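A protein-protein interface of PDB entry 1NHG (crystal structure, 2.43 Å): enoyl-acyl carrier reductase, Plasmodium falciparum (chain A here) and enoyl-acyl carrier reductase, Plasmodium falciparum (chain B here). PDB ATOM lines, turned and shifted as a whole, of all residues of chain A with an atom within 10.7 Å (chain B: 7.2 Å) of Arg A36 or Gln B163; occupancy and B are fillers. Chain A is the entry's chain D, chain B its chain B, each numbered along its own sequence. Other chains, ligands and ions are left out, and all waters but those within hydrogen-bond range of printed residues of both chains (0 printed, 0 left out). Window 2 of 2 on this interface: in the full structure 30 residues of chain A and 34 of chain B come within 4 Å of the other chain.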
ATOM      1  N   VAL A  29     -15.481  -8.013  11.848  1.00  0.00           N
ATOM      2  CA  VAL A  29     -16.912  -8.289  11.840  1.00  0.00           C
ATOM      3  C   VAL A  29     -17.251  -8.944  10.502  1.00  0.00           C
ATOM      4  O   VAL A  29     -18.073  -9.854  10.441  1.00  0.00           O
ATOM      5  CB  VAL A  29     -17.741  -6.996  12.018  1.00  0.00           C
ATOM      6  CG1 VAL A  29     -19.235  -7.311  11.926  1.00  0.00           C
ATOM      7  CG2 VAL A  29     -17.421  -6.363  13.355  1.00  0.00           C
ATOM      8  N   ALA A  30     -16.598  -8.491   9.435  1.00  0.00           N
ATOM      9  CA  ALA A  30     -16.824  -9.053   8.102  1.00  0.00           C
ATOM     10  C   ALA A  30     -16.368 -10.507   8.092  1.00  0.00           C
ATOM     11  O   ALA A  30     -16.990 -11.375   7.482  1.00  0.00           O
ATOM     12  CB  ALA A  30     -16.045  -8.264   7.057  1.00  0.00           C
ATOM     13  N   SER A  31     -15.264 -10.756   8.780  1.00  0.00           N
ATOM     14  CA  SER A  31     -14.692 -12.087   8.870  1.00  0.00           C
ATOM     15  C   SER A  31     -15.662 -13.046   9.570  1.00  0.00           C
ATOM     16  O   SER A  31     -15.805 -14.204   9.174  1.00  0.00           O
ATOM     17  CB  SER A  31     -13.366 -12.005   9.628  1.00  0.00           C
ATOM     18  OG  SER A  31     -12.710 -13.251   9.631  1.00  0.00           O
ATOM     19  N   PHE A  32     -16.337 -12.551  10.605  1.00  0.00           N
ATOM     20  CA  PHE A  32     -17.293 -13.352  11.358  1.00  0.00           C
ATOM     21  C   PHE A  32     -18.552 -13.689  10.547  1.00  0.00           C
ATOM     22  O   PHE A  32     -19.059 -14.813  10.617  1.00  0.00           O
ATOM     23  CB  PHE A  32     -17.696 -12.616  12.636  1.00  0.00           C
ATOM     24  CG  PHE A  32     -18.907 -13.191  13.300  1.00  0.00           C
ATOM     25  CD1 PHE A  32     -18.846 -14.423  13.941  1.00  0.00           C
ATOM     26  CD2 PHE A  32     -20.122 -12.515  13.256  1.00  0.00           C
ATOM     27  CE1 PHE A  32     -19.981 -14.975  14.531  1.00  0.00           C
ATOM     28  CE2 PHE A  32     -21.264 -13.059  13.841  1.00  0.00           C
ATOM     29  CZ  PHE A  32     -21.195 -14.287  14.478  1.00  0.00           C
ATOM     30  N   LEU A  33     -19.064 -12.716   9.792  1.00  0.00           N
ATOM     31  CA  LEU A  33     -20.262 -12.944   8.984  1.00  0.00           C
ATOM     32  C   LEU A  33     -20.008 -13.898   7.817  1.00  0.00           C
ATOM     33  O   LEU A  33     -20.919 -14.608   7.387  1.00  0.00           O
ATOM     34  CB  LEU A  33     -20.822 -11.613   8.465  1.00  0.00           C
ATOM     35  CG  LEU A  33     -21.563 -10.745   9.495  1.00  0.00           C
ATOM     36  CD1 LEU A  33     -21.732  -9.334   8.971  1.00  0.00           C
ATOM     37  CD2 LEU A  33     -22.914 -11.367   9.799  1.00  0.00           C
ATOM     38  N   LEU A  34     -18.774 -13.929   7.318  1.00  0.00           N
ATOM     39  CA  LEU A  34     -18.424 -14.816   6.207  1.00  0.00           C
ATOM     40  C   LEU A  34     -18.137 -16.267   6.621  1.00  0.00           C
ATOM     41  O   LEU A  34     -18.125 -17.165   5.774  1.00  0.00           O
ATOM     42  CB  LEU A  34     -17.213 -14.266   5.454  1.00  0.00           C
ATOM     43  CG  LEU A  34     -17.454 -12.975   4.670  1.00  0.00           C
ATOM     44  CD1 LEU A  34     -16.127 -12.446   4.133  1.00  0.00           C
ATOM     45  CD2 LEU A  34     -18.438 -13.243   3.541  1.00  0.00           C
ATOM     46  N   SER A  35     -17.904 -16.491   7.912  1.00  0.00           N
ATOM     47  CA  SER A  35     -17.608 -17.829   8.419  1.00  0.00           C
ATOM     48  C   SER A  35     -18.879 -18.564   8.837  1.00  0.00           C
ATOM     49  O   SER A  35     -19.951 -17.964   8.927  1.00  0.00           O
ATOM     50  CB  SER A  35     -16.665 -17.739   9.619  1.00  0.00           C
ATOM     51  OG  SER A  35     -17.333 -17.194  10.744  1.00  0.00           O
ATOM     52  N   ARG A  36     -18.758 -19.861   9.097  1.00  0.00           N
ATOM     53  CA  ARG A  36     -19.911 -20.659   9.502  1.00  0.00           C
ATOM     54  C   ARG A  36     -20.358 -20.353  10.923  1.00  0.00           C
ATOM     55  O   ARG A  36     -21.383 -20.846  11.369  1.00  0.00           O
ATOM     56  CB  ARG A  36     -19.617 -22.156   9.372  1.00  0.00           C
ATOM     57  CG  ARG A  36     -19.629 -22.669   7.930  1.00  0.00           C
ATOM     58  CD  ARG A  36     -20.404 -23.994   7.809  1.00  0.00           C
ATOM     59  NE  ARG A  36     -19.847 -25.051   8.659  1.00  0.00           N
ATOM     60  CZ  ARG A  36     -20.352 -26.280   8.766  1.00  0.00           C
ATOM     61  NH1 ARG A  36     -21.435 -26.621   8.079  1.00  0.00           N
ATOM     62  NH2 ARG A  36     -19.769 -27.172   9.557  1.00  0.00           N
ATOM     63  N   GLU A  37     -19.595 -19.533  11.631  1.00  0.00           N
ATOM     64  CA  GLU A  37     -19.953 -19.170  12.996  1.00  0.00           C
ATOM     65  C   GLU A  37     -21.252 -18.365  13.024  1.00  0.00           C
ATOM     66  O   GLU A  37     -21.872 -18.214  14.073  1.00  0.00           O
ATOM     67  CB  GLU A  37     -18.832 -18.348  13.641  1.00  0.00           C
ATOM     68  CG  GLU A  37     -17.539 -19.117  13.907  1.00  0.00           C
ATOM     69  CD  GLU A  37     -17.703 -20.200  14.967  1.00  0.00           C
ATOM     70  OE1 GLU A  37     -18.393 -21.209  14.694  1.00  0.00           O
ATOM     71  OE2 GLU A  37     -17.149 -20.040  16.079  1.00  0.00           O
ATOM     72  N   SER A  38     -21.660 -17.845  11.872  1.00  0.00           N
ATOM     73  CA  SER A  38     -22.882 -17.051  11.786  1.00  0.00           C
ATOM     74  C   SER A  38     -23.886 -17.683  10.826  1.00  0.00           C
ATOM     75  O   SER A  38     -24.591 -16.978  10.101  1.00  0.00           O
ATOM     76  CB  SER A  38     -22.548 -15.633  11.316  1.00  0.00           C
ATOM     77  OG  SER A  38     -21.993 -15.650  10.014  1.00  0.00           O
ATOM     78  N   ARG A  39     -23.950 -19.010  10.837  1.00  0.00           N
ATOM     79  CA  ARG A  39     -24.845 -19.762   9.963  1.00  0.00           C
ATOM     80  C   ARG A  39     -26.322 -19.394  10.093  1.00  0.00           C
ATOM     81  O   ARG A  39     -27.107 -19.675   9.183  1.00  0.00           O
ATOM     82  CB  ARG A  39     -24.681 -21.264  10.220  1.00  0.00           C
ATOM     83  CG  ARG A  39     -25.082 -21.696  11.625  1.00  0.00           C
ATOM     84  CD  ARG A  39     -24.647 -23.128  11.923  1.00  0.00           C
ATOM     85  NE  ARG A  39     -25.323 -24.123  11.091  1.00  0.00           N
ATOM     86  CZ  ARG A  39     -26.477 -24.710  11.398  1.00  0.00           C
ATOM     87  NH1 ARG A  39     -27.103 -24.410  12.528  1.00  0.00           N
ATOM     88  NH2 ARG A  39     -27.004 -25.604  10.572  1.00  0.00           N
ATOM     89  N   ALA A  40     -26.698 -18.766  11.210  1.00  0.00           N
ATOM     90  CA  ALA A  40     -28.095 -18.399  11.438  1.00  0.00           C
ATOM     91  C   ALA A  40     -28.453 -16.942  11.155  1.00  0.00           C
ATOM     92  O   ALA A  40     -29.592 -16.524  11.391  1.00  0.00           O
ATOM     93  CB  ALA A  40     -28.495 -18.755  12.863  1.00  0.00           C
ATOM     94  N   ILE A  41     -27.497 -16.171  10.645  1.00  0.00           N
ATOM     95  CA  ILE A  41     -27.741 -14.767  10.344  1.00  0.00           C
ATOM     96  C   ILE A  41     -27.760 -14.504   8.838  1.00  0.00           C
ATOM     97  O   ILE A  41     -26.806 -14.823   8.133  1.00  0.00           O
ATOM     98  CB  ILE A  41     -26.659 -13.879  10.964  1.00  0.00           C
ATOM     99  CG1 ILE A  41     -26.614 -14.086  12.481  1.00  0.00           C
ATOM    100  CG2 ILE A  41     -26.938 -12.419  10.637  1.00  0.00           C
ATOM    101  CD1 ILE A  41     -25.494 -13.297  13.159  1.00  0.00           C
ATOM    102  N   THR A  42     -28.845 -13.917   8.345  1.00  0.00           N
ATOM    103  CA  THR A  42     -28.932 -13.613   6.926  1.00  0.00           C
ATOM    104  C   THR A  42     -29.967 -12.523   6.658  1.00  0.00           C
ATOM    105  O   THR A  42     -30.963 -12.413   7.378  1.00  0.00           O
ATOM    106  CB  THR A  42     -29.273 -14.885   6.090  1.00  0.00           C
ATOM    107  OG1 THR A  42     -28.954 -14.646   4.719  1.00  0.00           O
ATOM    108  CG2 THR A  42     -30.753 -15.235   6.181  1.00  0.00           C
ATOM    109  N   ARG B  26      -7.273 -15.611   9.380  1.00  0.00           N
ATOM    110  CA  ARG B  26      -7.923 -16.917   9.461  1.00  0.00           C
ATOM    111  C   ARG B  26      -7.500 -17.853   8.332  1.00  0.00           C
ATOM    112  O   ARG B  26      -8.115 -18.897   8.107  1.00  0.00           O
ATOM    113  CB  ARG B  26      -9.447 -16.746   9.466  1.00  0.00           C
ATOM    114  CG  ARG B  26      -9.921 -15.735  10.495  1.00  0.00           C
ATOM    115  CD  ARG B  26     -11.419 -15.806  10.716  1.00  0.00           C
ATOM    116  NE  ARG B  26     -11.878 -14.800  11.674  1.00  0.00           N
ATOM    117  CZ  ARG B  26     -13.107 -14.762  12.183  1.00  0.00           C
ATOM    118  NH1 ARG B  26     -14.003 -15.676  11.828  1.00  0.00           N
ATOM    119  NH2 ARG B  26     -13.446 -13.804  13.043  1.00  0.00           N
ATOM    120  N   ASN B 114     -16.081 -19.857  -1.562  1.00  0.00           N
ATOM    121  CA  ASN B 114     -17.146 -19.865  -0.567  1.00  0.00           C
ATOM    122  C   ASN B 114     -17.329 -18.548   0.180  1.00  0.00           C
ATOM    123  O   ASN B 114     -18.026 -18.489   1.194  1.00  0.00           O
ATOM    124  CB  ASN B 114     -16.902 -21.005   0.427  1.00  0.00           C
ATOM    125  CG  ASN B 114     -15.621 -20.826   1.228  1.00  0.00           C
ATOM    126  OD1 ASN B 114     -14.657 -20.212   0.771  1.00  0.00           O
ATOM    127  ND2 ASN B 114     -15.602 -21.385   2.426  1.00  0.00           N
ATOM    128  N   MET B 115     -16.712 -17.488  -0.325  1.00  0.00           N
ATOM    129  CA  MET B 115     -16.824 -16.183   0.310  1.00  0.00           C
ATOM    130  C   MET B 115     -16.784 -15.080  -0.729  1.00  0.00           C
ATOM    131  O   MET B 115     -15.859 -15.010  -1.538  1.00  0.00           O
ATOM    132  CB  MET B 115     -15.689 -15.974   1.312  1.00  0.00           C
ATOM    133  CG  MET B 115     -15.697 -16.949   2.467  1.00  0.00           C
ATOM    134  SD  MET B 115     -14.485 -16.502   3.726  1.00  0.00           S
ATOM    135  CE  MET B 115     -14.809 -17.771   5.009  1.00  0.00           C
ATOM    136  N   MET B 160     -20.069 -21.085  -6.285  1.00  0.00           N
ATOM    137  CA  MET B 160     -19.995 -21.070  -4.828  1.00  0.00           C
ATOM    138  C   MET B 160     -20.515 -22.360  -4.211  1.00  0.00           C
ATOM    139  O   MET B 160     -21.483 -22.949  -4.684  1.00  0.00           O
ATOM    140  CB  MET B 160     -20.782 -19.888  -4.257  1.00  0.00           C
ATOM    141  CG  MET B 160     -20.245 -18.530  -4.659  1.00  0.00           C
ATOM    142  SD  MET B 160     -20.993 -17.219  -3.695  1.00  0.00           S
ATOM    143  CE  MET B 160     -19.733 -17.011  -2.429  1.00  0.00           C
ATOM    144  N   LYS B 161     -19.858 -22.799  -3.148  1.00  0.00           N
ATOM    145  CA  LYS B 161     -20.269 -24.008  -2.471  1.00  0.00           C
ATOM    146  C   LYS B 161     -21.444 -23.679  -1.570  1.00  0.00           C
ATOM    147  O   LYS B 161     -21.635 -22.527  -1.181  1.00  0.00           O
ATOM    148  CB  LYS B 161     -19.105 -24.579  -1.653  1.00  0.00           C
ATOM    149  CG  LYS B 161     -18.069 -25.297  -2.515  1.00  0.00           C
ATOM    150  CD  LYS B 161     -16.885 -25.821  -1.714  1.00  0.00           C
ATOM    151  CE  LYS B 161     -15.945 -24.700  -1.305  1.00  0.00           C
ATOM    152  NZ  LYS B 161     -14.711 -25.222  -0.653  1.00  0.00           N
ATOM    153  N   PRO B 162     -22.266 -24.685  -1.245  1.00  0.00           N
ATOM    154  CA  PRO B 162     -23.421 -24.460  -0.374  1.00  0.00           C
ATOM    155  C   PRO B 162     -22.901 -23.928   0.954  1.00  0.00           C
ATOM    156  O   PRO B 162     -21.755 -24.192   1.319  1.00  0.00           O
ATOM    157  CB  PRO B 162     -24.023 -25.854  -0.228  1.00  0.00           C
ATOM    158  CG  PRO B 162     -23.600 -26.549  -1.495  1.00  0.00           C
ATOM    159  CD  PRO B 162     -22.184 -26.093  -1.666  1.00  0.00           C
ATOM    160  N   GLN B 163     -23.740 -23.180   1.664  1.00  0.00           N
ATOM    161  CA  GLN B 163     -23.369 -22.611   2.958  1.00  0.00           C
ATOM    162  C   GLN B 163     -22.337 -21.498   2.877  1.00  0.00           C
ATOM    163  O   GLN B 163     -21.806 -21.072   3.899  1.00  0.00           O
ATOM    164  CB  GLN B 163     -22.854 -23.700   3.898  1.00  0.00           C
ATOM    165  CG  GLN B 163     -23.912 -24.693   4.329  1.00  0.00           C
ATOM    166  CD  GLN B 163     -23.330 -25.823   5.146  1.00  0.00           C
ATOM    167  OE1 GLN B 163     -22.497 -26.594   4.660  1.00  0.00           O
ATOM    168  NE2 GLN B 163     -23.759 -25.931   6.401  1.00  0.00           N
ATOM    169  N   SER B 164     -22.045 -21.031   1.669  1.00  0.00           N
ATOM    170  CA  SER B 164     -21.089 -19.949   1.515  1.00  0.00           C
ATOM    171  C   SER B 164     -21.777 -18.661   1.967  1.00  0.00           C
ATOM    172  O   SER B 164     -23.001 -18.622   2.100  1.00  0.00           O
ATOM    173  CB  SER B 164     -20.618 -19.856   0.063  1.00  0.00           C
ATOM    174  OG  SER B 164     -21.705 -19.972  -0.831  1.00  0.00           O
ATOM    175  N   SER B 165     -20.994 -17.616   2.215  1.00  0.00           N
ATOM    176  CA  SER B 165     -21.529 -16.350   2.700  1.00  0.00           C
ATOM    177  C   SER B 165     -21.126 -15.153   1.828  1.00  0.00           C
ATOM    178  O   SER B 165     -20.048 -15.131   1.237  1.00  0.00           O
ATOM    179  CB  SER B 165     -21.056 -16.139   4.143  1.00  0.00           C
ATOM    180  OG  SER B 165     -21.741 -15.080   4.783  1.00  0.00           O
ATOM    181  N   TYR B 207     -30.005 -21.915  -2.953  1.00  0.00           N
ATOM    182  CA  TYR B 207     -28.622 -22.367  -2.865  1.00  0.00           C
ATOM    183  C   TYR B 207     -28.095 -22.550  -1.453  1.00  0.00           C
ATOM    184  O   TYR B 207     -26.956 -22.979  -1.264  1.00  0.00           O
ATOM    185  CB  TYR B 207     -27.736 -21.375  -3.616  1.00  0.00           C
ATOM    186  CG  TYR B 207     -28.285 -21.039  -4.975  1.00  0.00           C
ATOM    187  CD1 TYR B 207     -28.097 -21.899  -6.061  1.00  0.00           C
ATOM    188  CD2 TYR B 207     -29.047 -19.892  -5.170  1.00  0.00           C
ATOM    189  CE1 TYR B 207     -28.661 -21.622  -7.307  1.00  0.00           C
ATOM    190  CE2 TYR B 207     -29.616 -19.605  -6.411  1.00  0.00           C
ATOM    191  CZ  TYR B 207     -29.421 -20.474  -7.474  1.00  0.00           C
ATOM    192  OH  TYR B 207     -29.999 -20.199  -8.693  1.00  0.00           O
ATOM    193  N   ASN B 208     -28.916 -22.229  -0.464  1.00  0.00           N
ATOM    194  CA  ASN B 208     -28.493 -22.347   0.924  1.00  0.00           C
ATOM    195  C   ASN B 208     -27.307 -21.408   1.171  1.00  0.00           C
ATOM    196  O   ASN B 208     -26.367 -21.747   1.891  1.00  0.00           O
ATOM    197  CB  ASN B 208     -28.083 -23.787   1.229  1.00  0.00           C
ATOM    198  CG  ASN B 208     -28.656 -24.288   2.539  1.00  0.00           C
ATOM    199  OD1 ASN B 208     -29.866 -24.517   2.650  1.00  0.00           O
ATOM    200  ND2 ASN B 208     -27.795 -24.452   3.545  1.00  0.00           N
ATOM    201  N   ILE B 209     -27.350 -20.231   0.554  1.00  0.00           N
ATOM    202  CA  ILE B 209     -26.290 -19.245   0.703  1.00  0.00           C
ATOM    203  C   ILE B 209     -26.792 -18.048   1.504  1.00  0.00           C
ATOM    204  O   ILE B 209     -27.957 -17.650   1.394  1.00  0.00           O
ATOM    205  CB  ILE B 209     -25.773 -18.778  -0.682  1.00  0.00           C
ATOM    206  CG1 ILE B 209     -24.911 -19.883  -1.307  1.00  0.00           C
ATOM    207  CG2 ILE B 209     -24.968 -17.493  -0.545  1.00  0.00           C
ATOM    208  CD1 ILE B 209     -24.337 -19.536  -2.662  1.00  0.00           C
ATOM    209  N   ARG B 210     -25.909 -17.479   2.314  1.00  0.00           N
ATOM    210  CA  ARG B 210     -26.266 -16.338   3.147  1.00  0.00           C
ATOM    211  C   ARG B 210     -25.728 -15.026   2.588  1.00  0.00           C
ATOM    212  O   ARG B 210     -24.729 -15.003   1.860  1.00  0.00           O
ATOM    213  CB  ARG B 210     -25.742 -16.549   4.575  1.00  0.00           C
ATOM    214  CG  ARG B 210     -26.367 -17.749   5.285  1.00  0.00           C
ATOM    215  CD  ARG B 210     -25.924 -17.868   6.739  1.00  0.00           C
ATOM    216  NE  ARG B 210     -24.499 -18.144   6.868  1.00  0.00           N
ATOM    217  CZ  ARG B 210     -23.577 -17.237   7.176  1.00  0.00           C
ATOM    218  NH1 ARG B 210     -23.925 -15.976   7.394  1.00  0.00           N
ATOM    219  NH2 ARG B 210     -22.306 -17.594   7.275  1.00  0.00           N
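Among the printed residues, merely in contact across the chains: Arg A39 with Arg B210, Leu A34 with Ser B165, Leu A34 with Met B115, Thr A42 with Arg B210, Ser A35 with Arg B26 and Phe A32 with Arg B26.
NE of Arg B26 is in hydrogen-bond range of OG of Ser A31 (2.7 Å).
The side-chain amide nitrogen of Gln B163 lies close to the guanidinium group of Arg A36.
The side-chain hydroxyl (OG) of Ser B165 lies within hydrogen-bond range of the backbone carbonyl oxygen (O) of Leu A33 (2.8 Å).
The guanidinium group (NH2) of Arg B210 is in hydrogen-bond range of the backbone carbonyl oxygen (O) of Leu A33, 3.3 Å away.
O of Ser A35 lies within hydrogen-bond range of NH2 of Arg B210, 2.9 Å away.
The backbone carbonyl oxygen (O) of Ser A38 is in hydrogen-bond range of the guanidinium group (NH1) of Arg B210 (3.0 Å).
The backbone carbonyl oxygen (O) of Ile A41 sits at hydrogen-bond distance from the guanidinium group (NH1) of Arg B210 (3.2 Å).
O of Asn B114 sits at hydrogen-bond distance from N of Ser B165, 3.3 Å away.
The backbone NH (N) of Gln B163 sits at hydrogen-bond distance from the backbone carbonyl oxygen (O) of Asn B208 (3.0 Å).
The backbone NH (N) of Arg B210 lies within hydrogen-bond range of the backbone carbonyl oxygen (O) of Ser B164.
O of Phe A32 lies within hydrogen-bond range of OG of Ser A38 (3.1 Å).
The side-chain hydroxyl (OG) of Ser A38 is in hydrogen-bond range of the backbone carbonyl oxygen (O) of Leu A33, at 3.0 Å.
O of Ser A35 sits at hydrogen-bond distance from OG of Ser A38 (3.3 Å).
Of the 13 printed residues of chain B, 5 touch a printed residue of chain A.
Along chain B the printed residues that touch a printed residue of chain A span positions 26 to 210.
Hydrophobic or aromatic side chains of chain A that line the printed part of chain B: Leu A34.
Of the printed residues of chain B, Phe A32 touches Arg B26 (3.98 Å).
Of the printed residues of chain B, Leu A33 touches Ser B165 and Arg B210.
Printed residues of chain B within 4 Å of Ser A35: Arg B26 (3.8 Å) and Arg B210 (2.9 Å).
Of chain B, only Gln B163 (2.9 Å) comes within 4 Å of Arg A36.
Ala A40 touches none of the printed residues of chain B.
Of the printed residues of chain B, Ile A41 touches Arg B210 (3.2 Å).
Of the printed residues of chain A, Met B115 touches Leu A34 (3.5 Å).
Met B160 touches none of the printed residues of chain A.
No residue of chain A comes within 4 Å of Pro B162.
Ser B164 touches none of the printed residues of chain A.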
